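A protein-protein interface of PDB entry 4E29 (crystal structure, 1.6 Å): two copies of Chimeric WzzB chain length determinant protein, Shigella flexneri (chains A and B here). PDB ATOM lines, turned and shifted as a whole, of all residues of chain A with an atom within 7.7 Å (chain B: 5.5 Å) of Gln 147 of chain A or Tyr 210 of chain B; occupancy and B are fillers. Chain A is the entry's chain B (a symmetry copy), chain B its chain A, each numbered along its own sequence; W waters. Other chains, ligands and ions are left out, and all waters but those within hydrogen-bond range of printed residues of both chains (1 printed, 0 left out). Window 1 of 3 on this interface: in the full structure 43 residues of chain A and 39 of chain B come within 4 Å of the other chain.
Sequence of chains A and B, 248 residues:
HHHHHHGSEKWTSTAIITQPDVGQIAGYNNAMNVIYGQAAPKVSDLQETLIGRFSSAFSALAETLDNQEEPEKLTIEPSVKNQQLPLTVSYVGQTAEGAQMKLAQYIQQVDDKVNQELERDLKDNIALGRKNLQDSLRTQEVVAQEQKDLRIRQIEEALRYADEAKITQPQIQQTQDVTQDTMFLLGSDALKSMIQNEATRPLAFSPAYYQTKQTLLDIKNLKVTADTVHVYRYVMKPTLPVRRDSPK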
ATOM      1  N   GLN A 140     -35.742 -16.355  15.204  1.00  0.00           N
ATOM      2  CA  GLN A 140     -34.872 -16.517  16.362  1.00  0.00           C
ATOM      3  C   GLN A 140     -33.450 -16.777  15.903  1.00  0.00           C
ATOM      4  O   GLN A 140     -32.494 -16.298  16.521  1.00  0.00           O
ATOM      5  CB  GLN A 140     -35.354 -17.663  17.259  1.00  0.00           C
ATOM      6  CG  GLN A 140     -36.613 -17.312  18.033  1.00  0.00           C
ATOM      7  CD  GLN A 140     -37.013 -18.401  18.988  1.00  0.00           C
ATOM      8  OE1 GLN A 140     -36.288 -18.707  19.936  1.00  0.00           O
ATOM      9  NE2 GLN A 140     -38.171 -19.003  18.749  1.00  0.00           N
ATOM     10  N   GLU A 141     -33.307 -17.527  14.818  1.00  0.00           N
ATOM     11  CA  GLU A 141     -31.989 -17.811  14.250  1.00  0.00           C
ATOM     12  C   GLU A 141     -31.327 -16.556  13.688  1.00  0.00           C
ATOM     13  O   GLU A 141     -30.111 -16.403  13.744  1.00  0.00           O
ATOM     14  CB  GLU A 141     -32.103 -18.884  13.166  1.00  0.00           C
ATOM     15  CG  GLU A 141     -32.364 -20.257  13.729  1.00  0.00           C
ATOM     16  CD  GLU A 141     -33.123 -21.151  12.778  1.00  0.00           C
ATOM     17  OE2 GLU A 141     -33.586 -22.201  13.247  1.00  0.00           O
ATOM     18  N   VAL A 142     -32.128 -15.661  13.128  1.00  0.00           N
ATOM     19  CA  VAL A 142     -31.585 -14.390  12.663  1.00  0.00           C
ATOM     20  C   VAL A 142     -30.974 -13.641  13.845  1.00  0.00           C
ATOM     21  O   VAL A 142     -29.858 -13.132  13.759  1.00  0.00           O
ATOM     22  CB  VAL A 142     -32.653 -13.519  11.978  1.00  0.00           C
ATOM     23  CG1 VAL A 142     -32.133 -12.100  11.732  1.00  0.00           C
ATOM     24  CG2 VAL A 142     -33.108 -14.182  10.679  1.00  0.00           C
ATOM     25  N   VAL A 143     -31.693 -13.596  14.960  1.00  0.00           N
ATOM     26  CA  VAL A 143     -31.190 -12.932  16.160  1.00  0.00           C
ATOM     27  C   VAL A 143     -29.930 -13.628  16.693  1.00  0.00           C
ATOM     28  O   VAL A 143     -28.958 -12.964  17.060  1.00  0.00           O
ATOM     29  CB  VAL A 143     -32.282 -12.865  17.259  1.00  0.00           C
ATOM     30  CG1 VAL A 143     -31.680 -12.425  18.595  1.00  0.00           C
ATOM     31  CG2 VAL A 143     -33.411 -11.926  16.828  1.00  0.00           C
ATOM     32  N   ALA A 144     -29.945 -14.960  16.719  1.00  0.00           N
ATOM     33  CA  ALA A 144     -28.792 -15.714  17.201  1.00  0.00           C
ATOM     34  C   ALA A 144     -27.585 -15.439  16.312  1.00  0.00           C
ATOM     35  O   ALA A 144     -26.452 -15.334  16.799  1.00  0.00           O
ATOM     36  CB  ALA A 144     -29.102 -17.200  17.258  1.00  0.00           C
ATOM     37  N   GLN A 145     -27.824 -15.304  15.008  1.00  0.00           N
ATOM     38  CA  GLN A 145     -26.732 -14.977  14.092  1.00  0.00           C
ATOM     39  C   GLN A 145     -26.154 -13.592  14.378  1.00  0.00           C
ATOM     40  O   GLN A 145     -24.933 -13.401  14.340  1.00  0.00           O
ATOM     41  CB  GLN A 145     -27.183 -15.060  12.631  1.00  0.00           C
ATOM     42  CG  GLN A 145     -26.049 -14.781  11.649  1.00  0.00           C
ATOM     43  CD  GLN A 145     -25.048 -15.928  11.593  1.00  0.00           C
ATOM     44  OE1 GLN A 145     -25.440 -17.099  11.536  1.00  0.00           O
ATOM     45  NE2 GLN A 145     -23.759 -15.600  11.613  1.00  0.00           N
ATOM     46  N   GLU A 146     -27.022 -12.618  14.653  1.00  0.00           N
ATOM     47  CA  GLU A 146     -26.543 -11.267  14.956  1.00  0.00           C
ATOM     48  C   GLU A 146     -25.697 -11.302  16.224  1.00  0.00           C
ATOM     49  O   GLU A 146     -24.685 -10.611  16.338  1.00  0.00           O
ATOM     50  CB  GLU A 146     -27.715 -10.294  15.111  1.00  0.00           C
ATOM     51  CG  GLU A 146     -28.524 -10.109  13.846  1.00  0.00           C
ATOM     52  CD  GLU A 146     -29.623  -9.070  14.007  1.00  0.00           C
ATOM     53  OE2 GLU A 146     -29.290  -7.875  14.081  1.00  0.00           O
ATOM     54  N   GLN A 147     -26.116 -12.118  17.178  1.00  0.00           N
ATOM     55  CA  GLN A 147     -25.356 -12.244  18.417  1.00  0.00           C
ATOM     56  C   GLN A 147     -24.008 -12.902  18.186  1.00  0.00           C
ATOM     57  O   GLN A 147     -22.997 -12.469  18.764  1.00  0.00           O
ATOM     58  CB  GLN A 147     -26.163 -12.998  19.473  1.00  0.00           C
ATOM     59  CG  GLN A 147     -27.358 -12.174  19.965  1.00  0.00           C
ATOM     60  CD  GLN A 147     -28.376 -13.005  20.715  1.00  0.00           C
ATOM     61  OE1 GLN A 147     -28.439 -14.225  20.563  1.00  0.00           O
ATOM     62  NE2 GLN A 147     -29.188 -12.341  21.529  1.00  0.00           N
ATOM     63  N   LYS A 148     -23.972 -13.939  17.353  1.00  0.00           N
ATOM     64  CA  LYS A 148     -22.688 -14.549  16.999  1.00  0.00           C
ATOM     65  C   LYS A 148     -21.784 -13.542  16.281  1.00  0.00           C
ATOM     66  O   LYS A 148     -20.599 -13.434  16.589  1.00  0.00           O
ATOM     67  CB  LYS A 148     -22.891 -15.797  16.123  1.00  0.00           C
ATOM     68  CG  LYS A 148     -21.586 -16.298  15.480  1.00  0.00           C
ATOM     69  CD  LYS A 148     -21.850 -17.339  14.406  1.00  0.00           C
ATOM     70  CE  LYS A 148     -20.580 -17.690  13.661  1.00  0.00           C
ATOM     71  NZ  LYS A 148     -20.819 -18.906  12.815  1.00  0.00           N
ATOM     72  N   ASP A 149     -22.340 -12.803  15.324  1.00  0.00           N
ATOM     73  CA  ASP A 149     -21.549 -11.827  14.582  1.00  0.00           C
ATOM     74  C   ASP A 149     -20.940 -10.798  15.541  1.00  0.00           C
ATOM     75  O   ASP A 149     -19.786 -10.391  15.394  1.00  0.00           O
ATOM     76  CB  ASP A 149     -22.391 -11.132  13.508  1.00  0.00           C
ATOM     77  CG  ASP A 149     -22.770 -12.060  12.366  1.00  0.00           C
ATOM     78  OD1 ASP A 149     -22.181 -13.152  12.246  1.00  0.00           O
ATOM     79  OD2 ASP A 149     -23.673 -11.688  11.590  1.00  0.00           O
ATOM     80  N   LEU A 150     -21.698 -10.392  16.549  1.00  0.00           N
ATOM     81  CA  LEU A 150     -21.165  -9.415  17.492  1.00  0.00           C
ATOM     82  C   LEU A 150     -20.058 -10.051  18.350  1.00  0.00           C
ATOM     83  O   LEU A 150     -19.049  -9.409  18.647  1.00  0.00           O
ATOM     84  CB  LEU A 150     -22.285  -8.785  18.339  1.00  0.00           C
ATOM     85  CG  LEU A 150     -21.840  -7.636  19.263  1.00  0.00           C
ATOM     86  CD1 LEU A 150     -22.965  -6.616  19.428  1.00  0.00           C
ATOM     87  CD2 LEU A 150     -21.382  -8.192  20.607  1.00  0.00           C
ATOM     88  N   ARG A 151     -20.247 -11.314  18.733  1.00  0.00           N
ATOM     89  CA  ARG A 151     -19.238 -12.035  19.510  1.00  0.00           C
ATOM     90  C   ARG A 151     -17.927 -12.097  18.745  1.00  0.00           C
ATOM     91  O   ARG A 151     -16.867 -11.863  19.312  1.00  0.00           O
ATOM     92  CB  ARG A 151     -19.727 -13.445  19.844  1.00  0.00           C
ATOM     93  CG  ARG A 151     -18.772 -14.248  20.726  1.00  0.00           C
ATOM     94  CD  ARG A 151     -18.754 -13.679  22.105  1.00  0.00           C
ATOM     95  NE  ARG A 151     -18.215 -14.613  23.081  1.00  0.00           N
ATOM     96  CZ  ARG A 151     -18.486 -14.552  24.379  1.00  0.00           C
ATOM     97  NH1 ARG A 151     -19.303 -13.615  24.836  1.00  0.00           N
ATOM     98  NH2 ARG A 151     -17.947 -15.423  25.219  1.00  0.00           N
ATOM     99  N   ILE A 152     -17.997 -12.422  17.458  1.00  0.00           N
ATOM    100  CA  ILE A 152     -16.790 -12.416  16.630  1.00  0.00           C
ATOM    101  C   ILE A 152     -16.143 -11.036  16.621  1.00  0.00           C
ATOM    102  O   ILE A 152     -14.917 -10.913  16.688  1.00  0.00           O
ATOM    103  CB  ILE A 152     -17.102 -12.876  15.197  1.00  0.00           C
ATOM    104  CG1 ILE A 152     -17.601 -14.316  15.205  1.00  0.00           C
ATOM    105  CG2 ILE A 152     -15.891 -12.713  14.289  1.00  0.00           C
ATOM    106  CD1 ILE A 152     -16.597 -15.324  15.744  1.00  0.00           C
ATOM    107  N   ARG A 153     -16.942  -9.980  16.550  1.00  0.00           N
ATOM    108  CA  ARG A 153     -16.356  -8.644  16.623  1.00  0.00           C
ATOM    109  C   ARG A 153     -15.664  -8.411  17.971  1.00  0.00           C
ATOM    110  O   ARG A 153     -14.605  -7.788  18.027  1.00  0.00           O
ATOM    111  CB  ARG A 153     -17.411  -7.576  16.329  1.00  0.00           C
ATOM    112  CG  ARG A 153     -17.883  -7.609  14.874  1.00  0.00           C
ATOM    113  CD  ARG A 153     -16.885  -6.881  13.972  1.00  0.00           C
ATOM    114  NE  ARG A 153     -16.701  -5.551  14.521  1.00  0.00           N
ATOM    115  CZ  ARG A 153     -15.588  -5.095  15.091  1.00  0.00           C
ATOM    116  NH1 ARG A 153     -14.471  -5.824  15.142  1.00  0.00           N
ATOM    117  NH2 ARG A 153     -15.597  -3.873  15.589  1.00  0.00           N
ATOM    118  N   GLN A 154     -16.258  -8.903  19.057  1.00  0.00           N
ATOM    119  CA  GLN A 154     -15.620  -8.765  20.368  1.00  0.00           C
ATOM    120  C   GLN A 154     -14.286  -9.497  20.397  1.00  0.00           C
ATOM    121  O   GLN A 154     -13.316  -9.009  20.981  1.00  0.00           O
ATOM    122  CB  GLN A 154     -16.507  -9.294  21.487  1.00  0.00           C
ATOM    123  CG  GLN A 154     -17.784  -8.471  21.642  1.00  0.00           C
ATOM    124  CD  GLN A 154     -18.695  -9.019  22.710  1.00  0.00           C
ATOM    125  OE1 GLN A 154     -18.939 -10.217  22.776  1.00  0.00           O
ATOM    126  NE2 GLN A 154     -19.214  -8.132  23.561  1.00  0.00           N
ATOM    127  N   ARG A 201     -18.251 -21.862  13.444  1.00  0.00           N
ATOM    128  CA  ARG A 201     -18.622 -21.717  14.849  1.00  0.00           C
ATOM    129  C   ARG A 201     -20.148 -21.858  14.990  1.00  0.00           C
ATOM    130  O   ARG A 201     -20.888 -21.085  14.381  1.00  0.00           O
ATOM    131  CB  ARG A 201     -18.168 -20.344  15.355  1.00  0.00           C
ATOM    132  CG  ARG A 201     -18.518 -20.064  16.811  1.00  0.00           C
ATOM    133  CD  ARG A 201     -18.411 -18.578  17.151  1.00  0.00           C
ATOM    134  NE  ARG A 201     -18.728 -18.343  18.559  1.00  0.00           N
ATOM    135  CZ  ARG A 201     -17.834 -18.209  19.535  1.00  0.00           C
ATOM    136  NH1 ARG A 201     -16.529 -18.274  19.282  1.00  0.00           N
ATOM    137  NH2 ARG A 201     -18.253 -18.012  20.776  1.00  0.00           N
ATOM    138  N   LEU A 203     -23.973 -21.538  16.342  1.00  0.00           N
ATOM    139  CA  LEU A 203     -24.730 -20.483  17.000  1.00  0.00           C
ATOM    140  C   LEU A 203     -25.000 -20.838  18.466  1.00  0.00           C
ATOM    141  O   LEU A 203     -25.086 -22.018  18.814  1.00  0.00           O
ATOM    142  CB  LEU A 203     -26.054 -20.291  16.268  1.00  0.00           C
ATOM    143  CG  LEU A 203     -25.912 -19.761  14.843  1.00  0.00           C
ATOM    144  CD1 LEU A 203     -27.264 -19.682  14.163  1.00  0.00           C
ATOM    145  CD2 LEU A 203     -25.261 -18.395  14.862  1.00  0.00           C
ATOM    146  N   ALA A 204     -25.140 -19.825  19.318  1.00  0.00           N
ATOM    147  CA  ALA A 204     -25.465 -20.049  20.730  1.00  0.00           C
ATOM    148  C   ALA A 204     -26.977 -19.935  20.961  1.00  0.00           C
ATOM    149  O   ALA A 204     -27.510 -18.835  21.117  1.00  0.00           O
ATOM    150  CB  ALA A 204     -24.704 -19.060  21.617  1.00  0.00           C
ATOM    151  N   PHE A 205     -27.662 -21.072  20.972  1.00  0.00           N
ATOM    152  CA  PHE A 205     -29.119 -21.075  21.096  1.00  0.00           C
ATOM    153  C   PHE A 205     -29.576 -21.089  22.549  1.00  0.00           C
ATOM    154  O   PHE A 205     -28.952 -21.721  23.403  1.00  0.00           O
ATOM    155  CB  PHE A 205     -29.709 -22.264  20.354  1.00  0.00           C
ATOM    156  CG  PHE A 205     -29.626 -22.153  18.863  1.00  0.00           C
ATOM    157  CD1 PHE A 205     -30.288 -21.134  18.192  1.00  0.00           C
ATOM    158  CD2 PHE A 205     -28.910 -23.075  18.127  1.00  0.00           C
ATOM    159  CE1 PHE A 205     -30.223 -21.032  16.817  1.00  0.00           C
ATOM    160  CE2 PHE A 205     -28.850 -22.985  16.747  1.00  0.00           C
ATOM    161  CZ  PHE A 205     -29.510 -21.957  16.091  1.00  0.00           C
ATOM    162  N   SER A 206     -30.685 -20.410  22.818  1.00  0.00           N
ATOM    163  CA  SER A 206     -31.170 -20.238  24.181  1.00  0.00           C
ATOM    164  C   SER A 206     -32.194 -21.302  24.521  1.00  0.00           C
ATOM    165  O   SER A 206     -32.670 -22.014  23.635  1.00  0.00           O
ATOM    166  CB  SER A 206     -31.835 -18.875  24.322  1.00  0.00           C
ATOM    167  OG  SER A 206     -33.092 -18.881  23.671  1.00  0.00           O
ATOM    168  N   PHE B 205     -25.270  -5.185  24.469  1.00  0.00           N
ATOM    169  CA  PHE B 205     -26.723  -5.196  24.301  1.00  0.00           C
ATOM    170  C   PHE B 205     -27.364  -6.218  25.227  1.00  0.00           C
ATOM    171  O   PHE B 205     -26.863  -7.330  25.382  1.00  0.00           O
ATOM    172  CB  PHE B 205     -27.082  -5.512  22.857  1.00  0.00           C
ATOM    173  CG  PHE B 205     -26.784  -4.396  21.893  1.00  0.00           C
ATOM    174  CD1 PHE B 205     -27.420  -3.166  22.012  1.00  0.00           C
ATOM    175  CD2 PHE B 205     -25.903  -4.588  20.844  1.00  0.00           C
ATOM    176  CE1 PHE B 205     -27.169  -2.146  21.112  1.00  0.00           C
ATOM    177  CE2 PHE B 205     -25.646  -3.569  19.934  1.00  0.00           C
ATOM    178  CZ  PHE B 205     -26.288  -2.343  20.072  1.00  0.00           C
ATOM    179  N   SER B 206     -28.484  -5.833  25.832  1.00  0.00           N
ATOM    180  CA  SER B 206     -29.145  -6.653  26.839  1.00  0.00           C
ATOM    181  C   SER B 206     -30.127  -7.625  26.204  1.00  0.00           C
ATOM    182  O   SER B 206     -30.481  -7.480  25.035  1.00  0.00           O
ATOM    183  CB  SER B 206     -29.918  -5.753  27.795  1.00  0.00           C
ATOM    184  OG  SER B 206     -31.020  -5.171  27.122  1.00  0.00           O
ATOM    185  N   PRO B 207     -30.570  -8.628  26.975  1.00  0.00           N
ATOM    186  CA  PRO B 207     -31.624  -9.501  26.450  1.00  0.00           C
ATOM    187  C   PRO B 207     -32.854  -8.700  26.040  1.00  0.00           C
ATOM    188  O   PRO B 207     -33.496  -9.052  25.058  1.00  0.00           O
ATOM    189  CB  PRO B 207     -31.942 -10.413  27.641  1.00  0.00           C
ATOM    190  CG  PRO B 207     -30.658 -10.466  28.414  1.00  0.00           C
ATOM    191  CD  PRO B 207     -30.077  -9.081  28.287  1.00  0.00           C
ATOM    192  N   ALA B 208     -33.172  -7.632  26.766  1.00  0.00           N
ATOM    193  CA  ALA B 208     -34.354  -6.838  26.443  1.00  0.00           C
ATOM    194  C   ALA B 208     -34.226  -6.208  25.057  1.00  0.00           C
ATOM    195  O   ALA B 208     -35.190  -6.143  24.290  1.00  0.00           O
ATOM    196  CB  ALA B 208     -34.606  -5.776  27.508  1.00  0.00           C
ATOM    197  N   TYR B 209     -33.016  -5.770  24.726  1.00  0.00           N
ATOM    198  CA  TYR B 209     -32.753  -5.211  23.409  1.00  0.00           C
ATOM    199  C   TYR B 209     -33.016  -6.249  22.323  1.00  0.00           C
ATOM    200  O   TYR B 209     -33.644  -5.960  21.306  1.00  0.00           O
ATOM    201  CB  TYR B 209     -31.309  -4.715  23.330  1.00  0.00           C
ATOM    202  CG  TYR B 209     -30.896  -4.233  21.963  1.00  0.00           C
ATOM    203  CD1 TYR B 209     -31.144  -2.927  21.560  1.00  0.00           C
ATOM    204  CD2 TYR B 209     -30.250  -5.082  21.075  1.00  0.00           C
ATOM    205  CE1 TYR B 209     -30.760  -2.475  20.321  1.00  0.00           C
ATOM    206  CE2 TYR B 209     -29.861  -4.643  19.822  1.00  0.00           C
ATOM    207  CZ  TYR B 209     -30.117  -3.343  19.449  1.00  0.00           C
ATOM    208  OH  TYR B 209     -29.735  -2.900  18.210  1.00  0.00           O
ATOM    209  N   TYR B 210     -32.550  -7.472  22.537  1.00  0.00           N
ATOM    210  CA  TYR B 210     -32.739  -8.510  21.529  1.00  0.00           C
ATOM    211  C   TYR B 210     -34.183  -9.000  21.446  1.00  0.00           C
ATOM    212  O   TYR B 210     -34.616  -9.486  20.401  1.00  0.00           O
ATOM    213  CB  TYR B 210     -31.765  -9.661  21.744  1.00  0.00           C
ATOM    214  CG  TYR B 210     -30.361  -9.292  21.333  1.00  0.00           C
ATOM    215  CD1 TYR B 210     -30.057  -9.073  20.000  1.00  0.00           C
ATOM    216  CD2 TYR B 210     -29.345  -9.154  22.277  1.00  0.00           C
ATOM    217  CE1 TYR B 210     -28.777  -8.731  19.603  1.00  0.00           C
ATOM    218  CE2 TYR B 210     -28.054  -8.810  21.896  1.00  0.00           C
ATOM    219  CZ  TYR B 210     -27.778  -8.604  20.553  1.00  0.00           C
ATOM    220  OH  TYR B 210     -26.506  -8.264  20.159  1.00  0.00           O
ATOM    221  N   GLN B 211     -34.919  -8.864  22.543  1.00  0.00           N
ATOM    222  CA  GLN B 211     -36.355  -9.134  22.527  1.00  0.00           C
ATOM    223  C   GLN B 211     -37.064  -8.129  21.618  1.00  0.00           C
ATOM    224  O   GLN B 211     -37.986  -8.479  20.874  1.00  0.00           O
ATOM    225  CB  GLN B 211     -36.925  -9.075  23.941  1.00  0.00           C
ATOM    226  N   THR B 212     -36.633  -6.874  21.675  1.00  0.00           N
ATOM    227  CA  THR B 212     -37.162  -5.856  20.779  1.00  0.00           C
ATOM    228  C   THR B 212     -36.883  -6.216  19.313  1.00  0.00           C
ATOM    229  O   THR B 212     -37.778  -6.146  18.468  1.00  0.00           O
ATOM    230  CB  THR B 212     -36.591  -4.463  21.122  1.00  0.00           C
ATOM    231  OG1 THR B 212     -36.851  -4.169  22.502  1.00  0.00           O
ATOM    232  CG2 THR B 212     -37.210  -3.389  20.247  1.00  0.00           C
ATOM    233  N   LYS B 213     -35.654  -6.629  19.011  1.00  0.00           N
ATOM    234  CA  LYS B 213     -35.317  -7.048  17.653  1.00  0.00           C
ATOM    235  C   LYS B 213     -36.138  -8.255  17.214  1.00  0.00           C
ATOM    236  O   LYS B 213     -36.584  -8.327  16.071  1.00  0.00           O
ATOM    237  CB  LYS B 213     -33.826  -7.385  17.533  1.00  0.00           C
ATOM    238  CG  LYS B 213     -32.903  -6.232  17.850  1.00  0.00           C
ATOM    239  CD  LYS B 213     -31.480  -6.551  17.427  1.00  0.00           C
ATOM    240  CE  LYS B 213     -31.295  -6.318  15.940  1.00  0.00           C
ATOM    241  NZ  LYS B 213     -30.534  -5.070  15.673  1.00  0.00           N
ATOM    242  N   GLN B 214     -36.313  -9.209  18.122  1.00  0.00           N
ATOM    243  CA  GLN B 214     -37.098 -10.399  17.831  1.00  0.00           C
ATOM    244  C   GLN B 214     -38.524 -10.022  17.447  1.00  0.00           C
ATOM    245  O   GLN B 214     -39.056 -10.505  16.447  1.00  0.00           O
ATOM    246  CB  GLN B 214     -37.102 -11.344  19.037  1.00  0.00           C
ATOM    247  CG  GLN B 214     -37.941 -12.604  18.836  1.00  0.00           C
ATOM    248  CD  GLN B 214     -37.382 -13.535  17.783  1.00  0.00           C
ATOM    249  OE1 GLN B 214     -36.194 -13.879  17.809  1.00  0.00           O
ATOM    250  NE2 GLN B 214     -38.230 -13.968  16.867  1.00  0.00           N
ATOM    251  N   THR B 215     -39.130  -9.157  18.251  1.00  0.00           N
ATOM    252  CA  THR B 215     -40.503  -8.720  18.015  1.00  0.00           C
ATOM    253  C   THR B 215     -40.617  -7.995  16.683  1.00  0.00           C
ATOM    254  O   THR B 215     -41.578  -8.191  15.933  1.00  0.00           O
ATOM    255  CB  THR B 215     -40.975  -7.805  19.151  1.00  0.00           C
ATOM    256  OG1 THR B 215     -41.062  -8.561  20.366  1.00  0.00           O
HETATM  257  O   HOH W   1     -28.636  -7.352  16.389  1.00  0.00           O
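Water W1 lies within hydrogen-bond range of OE2 of Glu 146 of chain A (2.5 Å) and NZ of Lys 213 of chain B (3.1 Å).
Positions printed for both chains: 205 and 206.
Among the printed residues, pairs that only touch across the chains: Gln 140 of chain A with Gln 214 of chain B (3.3 Å), Val 143 of chain A with Tyr 210 of chain B (3.98 Å), Val 143 of chain A with Gln 214 of chain B (3.5 Å), Gln 147 of chain A with Tyr 210 of chain B (3.3 Å), Leu 150 of chain A with Phe 205 of chain B (3.8 Å) and Leu 150 of chain A with Tyr 210 of chain B (3.97 Å).
Of the 20 printed residues of chain A, 5 touch a printed residue of chain B. Hydrophobic or aromatic side chains of chain A that line the printed part of chain B: Val 143 and Leu 150. Along chain B the printed residues that touch a printed residue of chain A span positions 205 to 214. Among the printed residues, Asp or Glu carboxylates within 4 Å of a Lys or Arg side-chain nitrogen of the other chain: Glu 146 of chain A with Lys 213 of chain B (3.5 Å).
OH of Tyr 209 of chain B sits at hydrogen-bond distance from NZ of Lys 213 of chain B.
Of the printed residues of chain B, Glu 146 of chain A touches Lys 213. Of chain B, only Tyr 210 comes within 4 Å of Gln 147 of chain A. Of the printed residues of chain B, Leu 150 of chain A touches Phe 205 and Tyr 210. Of the printed residues of chain A, Phe 205 of chain B touches Leu 150. Printed residues of chain A within 4 Å of Tyr 210 of chain B: Val 143, Gln 147 and Leu 150. The nearest printed residue of chain B that does not touch Gln 147 of chain A is Ser 206 of chain B (6.1 Å). The nearest printed residue of chain A that does not touch Tyr 210 of chain B is Glu 146 of chain A (4.8 Å).
The side-chain carboxylate of Glu 146 of chain A is in salt-bridge range of the side-chain amino group of Lys 213 of chain B (3.5 Å).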
